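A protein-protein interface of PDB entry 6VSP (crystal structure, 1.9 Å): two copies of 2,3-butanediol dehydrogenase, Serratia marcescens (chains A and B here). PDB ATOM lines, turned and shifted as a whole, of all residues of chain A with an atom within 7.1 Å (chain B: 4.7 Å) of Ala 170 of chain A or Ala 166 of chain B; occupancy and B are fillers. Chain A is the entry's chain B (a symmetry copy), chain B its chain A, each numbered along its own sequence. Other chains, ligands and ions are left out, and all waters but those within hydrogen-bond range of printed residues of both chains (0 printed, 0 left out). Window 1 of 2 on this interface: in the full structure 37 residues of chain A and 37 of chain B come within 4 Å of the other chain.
Ala 170 of chain A touches three residues of chain B. Of chain A, only Ala 170 (3.3 Å) and Leu 174 (3.9 Å) come within 4 Å of Ala 166 of chain B. Of the printed residues of chain A, Trp 117 of chain B touches Ile 125 (3.6 Å) and Val 129 (3.9 Å). Printed residues of chain A within 4 Å of Ala 162 of chain B: Leu 174. Val 172 of chain A touches none of the printed residues of chain B. Arg 176 of chain A touches none of the printed residues of chain B. The nearest printed residue of chain B that does not touch Ala 170 of chain A is Ala 167 of chain B (5.1 Å). The nearest printed residue of chain A that does not touch Cys 165 of chain B is Leu 174 of chain A (4.9 Å).
Among the printed residues, merely in contact across the chains: Ala 166 of chain A with Ala 170 of chain B (3.2 Å), Ala 170 of chain A with Ala 166 of chain B (3.3 Å), Ala 177 of chain A with Cys 165 of chain B (3.6 Å), Ile 125 of chain A with Trp 117 of chain B (3.6 Å), Val 129 of chain A with Tyr 163 of chain B (3.7 Å), Gly 169 of chain A with Gly 169 of chain B (3.7 Å), Ala 170 of chain A with Ala 170 of chain B (3.8 Å), Leu 174 of chain A with Ala 162 of chain B (3.8 Å), Asn 173 of chain A with Gly 169 of chain B (3.9 Å), Leu 174 of chain A with Ala 166 of chain B (3.9 Å), Val 129 of chain A with Trp 117 of chain B (3.9 Å) and Ala 170 of chain A with Gly 169 of chain B (3.9 Å).
The guanidinium group of Arg 176 of chain A is in hydrogen-bond range of the side-chain amide oxygen of Asn 173 of chain A, 2.8 Å away.
Of the 10 printed residues of chain B, 7 touch a printed residue of chain A. Of the 19 printed residues of chain A, 8 touch a printed residue of chain B. Along chain A the printed residues that touch a printed residue of chain B span positions 125 to 177. Among the printed residues, no Asp or Glu carboxylate lies within 4 Å of a Lys or Arg side-chain nitrogen of the other chain.
Ala 166 of chain A touches Ala 170 of chain B, and with the chains exchanged Ala 170 of chain A touches Ala 166 of chain B. Gly 169 of chain B touches its own counterpart, Gly 169 of chain A. Ala 170 of chain A touches Gly 169 of chain B, but with the chains exchanged Gly 169 of chain A does not touch Ala 170 of chain B (4.04 Å). Ala 170 of chain A touches its own counterpart, Ala 170 of chain B. 7 positions are printed for both chains. Of the 13 pairs that touch across the chains among the printed residues, 4 have their exchanged pair printed and touching as well.
The backbone carbonyl oxygen of Cys 165 of chain B lies within hydrogen-bond range of the side-chain amide nitrogen of Asn 173 of chain A (3.1 Å).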
ATOM      1  N   ASP A 124      23.678 -30.016  -0.126  1.00  0.00           N
ATOM      2  CA  ASP A 124      23.558 -28.582   0.254  1.00  0.00           C
ATOM      3  C   ASP A 124      22.390 -27.924  -0.483  1.00  0.00           C
ATOM      4  O   ASP A 124      21.863 -26.956   0.074  1.00  0.00           O
ATOM      5  CB  ASP A 124      24.845 -27.778   0.056  1.00  0.00           C
ATOM      6  CG  ASP A 124      25.999 -28.192   0.954  1.00  0.00           C
ATOM      7  OD1 ASP A 124      25.749 -28.914   1.879  1.00  0.00           O
ATOM      8  OD2 ASP A 124      27.156 -27.793   0.691  1.00  0.00           O
ATOM      9  N   ILE A 125      22.049 -28.369  -1.694  1.00  0.00           N
ATOM     10  CA  ILE A 125      20.933 -27.767  -2.467  1.00  0.00           C
ATOM     11  C   ILE A 125      19.751 -28.731  -2.429  1.00  0.00           C
ATOM     12  O   ILE A 125      18.675 -28.305  -1.953  1.00  0.00           O
ATOM     13  CB  ILE A 125      21.306 -27.393  -3.907  1.00  0.00           C
ATOM     14  CG1 ILE A 125      22.678 -26.721  -4.000  1.00  0.00           C
ATOM     15  CG2 ILE A 125      20.196 -26.551  -4.527  1.00  0.00           C
ATOM     16  CD1 ILE A 125      23.101 -26.455  -5.409  1.00  0.00           C
ATOM     17  N   VAL A 128      17.917 -29.253   0.887  1.00  0.00           N
ATOM     18  CA  VAL A 128      17.017 -28.132   1.289  1.00  0.00           C
ATOM     19  C   VAL A 128      15.745 -28.164   0.423  1.00  0.00           C
ATOM     20  O   VAL A 128      14.639 -28.074   1.006  1.00  0.00           O
ATOM     21  CB  VAL A 128      17.726 -26.783   1.217  1.00  0.00           C
ATOM     22  CG1 VAL A 128      16.771 -25.671   1.584  1.00  0.00           C
ATOM     23  CG2 VAL A 128      18.946 -26.753   2.144  1.00  0.00           C
ATOM     24  N   VAL A 129      15.874 -28.335  -0.907  1.00  0.00           N
ATOM     25  CA  VAL A 129      14.684 -28.395  -1.801  1.00  0.00           C
ATOM     26  C   VAL A 129      13.760 -29.525  -1.310  1.00  0.00           C
ATOM     27  O   VAL A 129      12.544 -29.295  -1.056  1.00  0.00           O
ATOM     28  CB  VAL A 129      15.062 -28.581  -3.281  1.00  0.00           C
ATOM     29  CG1 VAL A 129      13.821 -28.817  -4.134  1.00  0.00           C
ATOM     30  CG2 VAL A 129      15.897 -27.449  -3.860  1.00  0.00           C
ATOM     31  N   GLY A 154      27.068 -18.231   1.283  1.00  0.00           N
ATOM     32  CA  GLY A 154      25.929 -18.075   0.369  1.00  0.00           C
ATOM     33  C   GLY A 154      25.577 -16.626   0.122  1.00  0.00           C
ATOM     34  O   GLY A 154      24.836 -16.372  -0.864  1.00  0.00           O
ATOM     35  N   TYR A 164      30.807 -24.900  -3.307  1.00  0.00           N
ATOM     36  CA  TYR A 164      30.178 -24.664  -1.985  1.00  0.00           C
ATOM     37  C   TYR A 164      29.440 -23.315  -2.015  1.00  0.00           C
ATOM     38  O   TYR A 164      28.303 -23.234  -1.562  1.00  0.00           O
ATOM     39  CB  TYR A 164      31.223 -24.660  -0.867  1.00  0.00           C
ATOM     40  CG  TYR A 164      30.666 -24.519   0.521  1.00  0.00           C
ATOM     41  CD1 TYR A 164      29.956 -25.551   1.130  1.00  0.00           C
ATOM     42  CD2 TYR A 164      30.879 -23.367   1.247  1.00  0.00           C
ATOM     43  CE1 TYR A 164      29.471 -25.439   2.421  1.00  0.00           C
ATOM     44  CE2 TYR A 164      30.386 -23.226   2.534  1.00  0.00           C
ATOM     45  CZ  TYR A 164      29.690 -24.265   3.125  1.00  0.00           C
ATOM     46  OH  TYR A 164      29.201 -24.090   4.383  1.00  0.00           O
ATOM     47  N   CYS A 165      30.095 -22.282  -2.524  1.00  0.00           N
ATOM     48  CA  CYS A 165      29.515 -20.925  -2.663  1.00  0.00           C
ATOM     49  C   CYS A 165      28.296 -20.942  -3.599  1.00  0.00           C
ATOM     50  O   CYS A 165      27.310 -20.307  -3.245  1.00  0.00           O
ATOM     51  CB  CYS A 165      30.565 -19.957  -3.158  1.00  0.00           C
ATOM     52  SG  CYS A 165      31.720 -19.513  -1.838  1.00  0.00           S
ATOM     53  N   ALA A 166      28.365 -21.623  -4.729  1.00  0.00           N
ATOM     54  CA  ALA A 166      27.213 -21.818  -5.631  1.00  0.00           C
ATOM     55  C   ALA A 166      26.055 -22.451  -4.854  1.00  0.00           C
ATOM     56  O   ALA A 166      24.915 -21.963  -4.952  1.00  0.00           O
ATOM     57  CB  ALA A 166      27.610 -22.614  -6.833  1.00  0.00           C
ATOM     58  N   ALA A 167      26.310 -23.506  -4.094  1.00  0.00           N
ATOM     59  CA  ALA A 167      25.248 -24.272  -3.403  1.00  0.00           C
ATOM     60  C   ALA A 167      24.646 -23.388  -2.306  1.00  0.00           C
ATOM     61  O   ALA A 167      23.417 -23.303  -2.208  1.00  0.00           O
ATOM     62  CB  ALA A 167      25.803 -25.571  -2.845  1.00  0.00           C
ATOM     63  N   LYS A 168      25.471 -22.745  -1.493  1.00  0.00           N
ATOM     64  CA  LYS A 168      24.953 -21.877  -0.420  1.00  0.00           C
ATOM     65  C   LYS A 168      24.257 -20.646  -1.032  1.00  0.00           C
ATOM     66  O   LYS A 168      23.276 -20.143  -0.390  1.00  0.00           O
ATOM     67  CB  LYS A 168      26.069 -21.551   0.568  1.00  0.00           C
ATOM     68  CG  LYS A 168      26.502 -22.739   1.419  1.00  0.00           C
ATOM     69  CD  LYS A 168      25.386 -23.373   2.254  1.00  0.00           C
ATOM     70  CE  LYS A 168      25.897 -24.498   3.142  1.00  0.00           C
ATOM     71  NZ  LYS A 168      24.787 -25.170   3.862  1.00  0.00           N
ATOM     72  N   GLY A 169      24.709 -20.166  -2.189  1.00  0.00           N
ATOM     73  CA  GLY A 169      23.996 -19.083  -2.897  1.00  0.00           C
ATOM     74  C   GLY A 169      22.581 -19.512  -3.272  1.00  0.00           C
ATOM     75  O   GLY A 169      21.649 -18.714  -3.132  1.00  0.00           O
ATOM     76  N   ALA A 170      22.427 -20.765  -3.717  1.00  0.00           N
ATOM     77  CA  ALA A 170      21.131 -21.384  -4.044  1.00  0.00           C
ATOM     78  C   ALA A 170      20.232 -21.409  -2.803  1.00  0.00           C
ATOM     79  O   ALA A 170      19.048 -21.043  -2.909  1.00  0.00           O
ATOM     80  CB  ALA A 170      21.332 -22.762  -4.633  1.00  0.00           C
ATOM     81  N   VAL A 171      20.767 -21.775  -1.646  1.00  0.00           N
ATOM     82  CA  VAL A 171      19.957 -21.904  -0.400  1.00  0.00           C
ATOM     83  C   VAL A 171      19.460 -20.510   0.004  1.00  0.00           C
ATOM     84  O   VAL A 171      18.308 -20.367   0.418  1.00  0.00           O
ATOM     85  CB  VAL A 171      20.760 -22.583   0.726  1.00  0.00           C
ATOM     86  CG1 VAL A 171      19.981 -22.628   2.029  1.00  0.00           C
ATOM     87  CG2 VAL A 171      21.202 -23.972   0.311  1.00  0.00           C
ATOM     88  N   VAL A 172      20.335 -19.528  -0.047  1.00  0.00           N
ATOM     89  CA  VAL A 172      20.006 -18.139   0.351  1.00  0.00           C
ATOM     90  C   VAL A 172      18.840 -17.637  -0.521  1.00  0.00           C
ATOM     91  O   VAL A 172      17.918 -17.037   0.029  1.00  0.00           O
ATOM     92  CB  VAL A 172      21.260 -17.265   0.238  1.00  0.00           C
ATOM     93  CG1 VAL A 172      20.966 -15.794   0.067  1.00  0.00           C
ATOM     94  CG2 VAL A 172      22.156 -17.492   1.431  1.00  0.00           C
ATOM     95  N   ASN A 173      18.892 -17.827  -1.838  1.00  0.00           N
ATOM     96  CA  ASN A 173      17.847 -17.286  -2.737  1.00  0.00           C
ATOM     97  C   ASN A 173      16.615 -18.184  -2.702  1.00  0.00           C
ATOM     98  O   ASN A 173      15.496 -17.640  -2.842  1.00  0.00           O
ATOM     99  CB  ASN A 173      18.338 -16.981  -4.143  1.00  0.00           C
ATOM    100  CG  ASN A 173      17.579 -15.807  -4.733  1.00  0.00           C
ATOM    101  OD1 ASN A 173      17.426 -14.796  -4.046  1.00  0.00           O
ATOM    102  ND2 ASN A 173      17.034 -15.970  -5.936  1.00  0.00           N
ATOM    103  N   LEU A 174      16.763 -19.499  -2.532  1.00  0.00           N
ATOM    104  CA  LEU A 174      15.594 -20.390  -2.367  1.00  0.00           C
ATOM    105  C   LEU A 174      14.834 -19.994  -1.096  1.00  0.00           C
ATOM    106  O   LEU A 174      13.591 -20.012  -1.111  1.00  0.00           O
ATOM    107  CB  LEU A 174      16.064 -21.848  -2.294  1.00  0.00           C
ATOM    108  CG  LEU A 174      14.979 -22.911  -2.114  1.00  0.00           C
ATOM    109  CD1 LEU A 174      14.061 -23.068  -3.309  1.00  0.00           C
ATOM    110  CD2 LEU A 174      15.622 -24.263  -1.824  1.00  0.00           C
ATOM    111  N   THR A 175      15.544 -19.612  -0.024  1.00  0.00           N
ATOM    112  CA  THR A 175      14.933 -19.139   1.235  1.00  0.00           C
ATOM    113  C   THR A 175      14.016 -17.952   0.901  1.00  0.00           C
ATOM    114  O   THR A 175      12.858 -17.958   1.356  1.00  0.00           O
ATOM    115  CB  THR A 175      15.984 -18.723   2.269  1.00  0.00           C
ATOM    116  OG1 THR A 175      16.806 -19.851   2.534  1.00  0.00           O
ATOM    117  CG2 THR A 175      15.376 -18.200   3.541  1.00  0.00           C
ATOM    118  N   ARG A 176      14.518 -17.000   0.120  1.00  0.00           N
ATOM    119  CA  ARG A 176      13.719 -15.823  -0.325  1.00  0.00           C
ATOM    120  C   ARG A 176      12.471 -16.271  -1.100  1.00  0.00           C
ATOM    121  O   ARG A 176      11.361 -15.842  -0.744  1.00  0.00           O
ATOM    122  CB  ARG A 176      14.625 -14.916  -1.147  1.00  0.00           C
ATOM    123  CG  ARG A 176      15.749 -14.277  -0.321  1.00  0.00           C
ATOM    124  CD  ARG A 176      16.482 -13.282  -1.191  1.00  0.00           C
ATOM    125  NE  ARG A 176      17.707 -12.806  -0.572  1.00  0.00           N
ATOM    126  CZ  ARG A 176      18.938 -12.942  -1.059  1.00  0.00           C
ATOM    127  NH1 ARG A 176      19.938 -12.412  -0.380  1.00  0.00           N
ATOM    128  NH2 ARG A 176      19.194 -13.589  -2.193  1.00  0.00           N
ATOM    129  N   ALA A 177      12.654 -17.065  -2.140  1.00  0.00           N
ATOM    130  CA  ALA A 177      11.581 -17.437  -3.085  1.00  0.00           C
ATOM    131  C   ALA A 177      10.469 -18.196  -2.338  1.00  0.00           C
ATOM    132  O   ALA A 177       9.287 -17.851  -2.476  1.00  0.00           O
ATOM    133  CB  ALA A 177      12.166 -18.239  -4.209  1.00  0.00           C
ATOM    134  N   TRP B 117      12.619 -29.791 -11.224  1.00  0.00           N
ATOM    135  CA  TRP B 117      13.848 -29.362 -10.516  1.00  0.00           C
ATOM    136  C   TRP B 117      15.067 -29.789 -11.324  1.00  0.00           C
ATOM    137  O   TRP B 117      15.979 -28.958 -11.497  1.00  0.00           O
ATOM    138  CB  TRP B 117      13.888 -29.920  -9.102  1.00  0.00           C
ATOM    139  CG  TRP B 117      15.216 -29.758  -8.449  1.00  0.00           C
ATOM    140  CD1 TRP B 117      15.999 -30.753  -7.961  1.00  0.00           C
ATOM    141  CD2 TRP B 117      15.901 -28.536  -8.153  1.00  0.00           C
ATOM    142  NE1 TRP B 117      17.126 -30.228  -7.372  1.00  0.00           N
ATOM    143  CE2 TRP B 117      17.110 -28.880  -7.508  1.00  0.00           C
ATOM    144  CE3 TRP B 117      15.665 -27.192  -8.452  1.00  0.00           C
ATOM    145  CZ2 TRP B 117      18.041 -27.937  -7.104  1.00  0.00           C
ATOM    146  CZ3 TRP B 117      16.576 -26.253  -8.036  1.00  0.00           C
ATOM    147  CH2 TRP B 117      17.757 -26.624  -7.386  1.00  0.00           C
ATOM    148  N   ALA B 162      10.281 -21.029  -7.716  1.00  0.00           N
ATOM    149  CA  ALA B 162      11.206 -21.395  -6.612  1.00  0.00           C
ATOM    150  C   ALA B 162      12.485 -22.060  -7.160  1.00  0.00           C
ATOM    151  O   ALA B 162      13.597 -21.647  -6.786  1.00  0.00           O
ATOM    152  CB  ALA B 162      10.502 -22.272  -5.627  1.00  0.00           C
ATOM    153  N   TYR B 163      12.346 -23.068  -8.014  1.00  0.00           N
ATOM    154  CA  TYR B 163      13.504 -23.834  -8.529  1.00  0.00           C
ATOM    155  C   TYR B 163      14.405 -22.885  -9.322  1.00  0.00           C
ATOM    156  O   TYR B 163      15.644 -22.895  -9.142  1.00  0.00           O
ATOM    157  CB  TYR B 163      13.045 -25.001  -9.392  1.00  0.00           C
ATOM    158  CG  TYR B 163      12.270 -26.081  -8.681  1.00  0.00           C
ATOM    159  CD1 TYR B 163      12.326 -26.262  -7.302  1.00  0.00           C
ATOM    160  CD2 TYR B 163      11.457 -26.941  -9.411  1.00  0.00           C
ATOM    161  CE1 TYR B 163      11.611 -27.269  -6.672  1.00  0.00           C
ATOM    162  CE2 TYR B 163      10.716 -27.937  -8.791  1.00  0.00           C
ATOM    163  CZ  TYR B 163      10.810 -28.117  -7.424  1.00  0.00           C
ATOM    164  OH  TYR B 163      10.052 -29.068  -6.822  1.00  0.00           O
ATOM    165  N   TYR B 164      13.789 -22.052 -10.168  1.00  0.00           N
ATOM    166  CA  TYR B 164      14.486 -21.044 -11.015  1.00  0.00           C
ATOM    167  C   TYR B 164      15.286 -20.084 -10.125  1.00  0.00           C
ATOM    168  O   TYR B 164      16.445 -19.800 -10.413  1.00  0.00           O
ATOM    169  CB  TYR B 164      13.484 -20.277 -11.864  1.00  0.00           C
ATOM    170  CG  TYR B 164      14.077 -19.282 -12.814  1.00  0.00           C
ATOM    171  CD1 TYR B 164      14.686 -19.709 -13.984  1.00  0.00           C
ATOM    172  CD2 TYR B 164      13.933 -17.923 -12.611  1.00  0.00           C
ATOM    173  CE1 TYR B 164      15.193 -18.802 -14.908  1.00  0.00           C
ATOM    174  CE2 TYR B 164      14.433 -17.001 -13.522  1.00  0.00           C
ATOM    175  CZ  TYR B 164      15.058 -17.444 -14.672  1.00  0.00           C
ATOM    176  OH  TYR B 164      15.509 -16.560 -15.594  1.00  0.00           O
ATOM    177  N   CYS B 165      14.679 -19.608  -9.047  1.00  0.00           N
ATOM    178  CA  CYS B 165      15.335 -18.676  -8.093  1.00  0.00           C
ATOM    179  C   CYS B 165      16.533 -19.354  -7.405  1.00  0.00           C
ATOM    180  O   CYS B 165      17.600 -18.697  -7.256  1.00  0.00           O
ATOM    181  CB  CYS B 165      14.309 -18.171  -7.101  1.00  0.00           C
ATOM    182  SG  CYS B 165      13.231 -16.931  -7.864  1.00  0.00           S
ATOM    183  N   ALA B 166      16.385 -20.595  -6.962  1.00  0.00           N
ATOM    184  CA  ALA B 166      17.520 -21.369  -6.404  1.00  0.00           C
ATOM    185  C   ALA B 166      18.657 -21.444  -7.424  1.00  0.00           C
ATOM    186  O   ALA B 166      19.823 -21.160  -7.057  1.00  0.00           O
ATOM    187  CB  ALA B 166      17.061 -22.717  -5.971  1.00  0.00           C
ATOM    188  N   ALA B 167      18.349 -21.787  -8.674  1.00  0.00           N
ATOM    189  CA  ALA B 167      19.355 -21.953  -9.745  1.00  0.00           C
ATOM    190  C   ALA B 167      20.051 -20.625 -10.015  1.00  0.00           C
ATOM    191  O   ALA B 167      21.307 -20.588 -10.055  1.00  0.00           O
ATOM    192  CB  ALA B 167      18.733 -22.539 -10.990  1.00  0.00           C
ATOM    193  N   LYS B 168      19.288 -19.541 -10.178  1.00  0.00           N
ATOM    194  CA  LYS B 168      19.891 -18.240 -10.489  1.00  0.00           C
ATOM    195  C   LYS B 168      20.670 -17.736  -9.271  1.00  0.00           C
ATOM    196  O   LYS B 168      21.677 -17.029  -9.480  1.00  0.00           O
ATOM    197  CB  LYS B 168      18.821 -17.283 -11.019  1.00  0.00           C
ATOM    198  CG  LYS B 168      18.264 -17.642 -12.393  1.00  0.00           C
ATOM    199  CD  LYS B 168      19.323 -17.680 -13.462  1.00  0.00           C
ATOM    200  CE  LYS B 168      18.746 -17.738 -14.854  1.00  0.00           C
ATOM    201  NZ  LYS B 168      19.759 -17.945 -15.907  1.00  0.00           N
ATOM    202  N   GLY B 169      20.223 -18.034  -8.055  1.00  0.00           N
ATOM    203  CA  GLY B 169      20.988 -17.703  -6.842  1.00  0.00           C
ATOM    204  C   GLY B 169      22.355 -18.369  -6.852  1.00  0.00           C
ATOM    205  O   GLY B 169      23.335 -17.720  -6.445  1.00  0.00           O
ATOM    206  N   ALA B 170      22.412 -19.627  -7.309  1.00  0.00           N
ATOM    207  CA  ALA B 170      23.677 -20.374  -7.488  1.00  0.00           C
ATOM    208  C   ALA B 170      24.596 -19.632  -8.477  1.00  0.00           C
ATOM    209  O   ALA B 170      25.792 -19.490  -8.198  1.00  0.00           O
ATOM    210  CB  ALA B 170      23.396 -21.772  -7.933  1.00  0.00           C
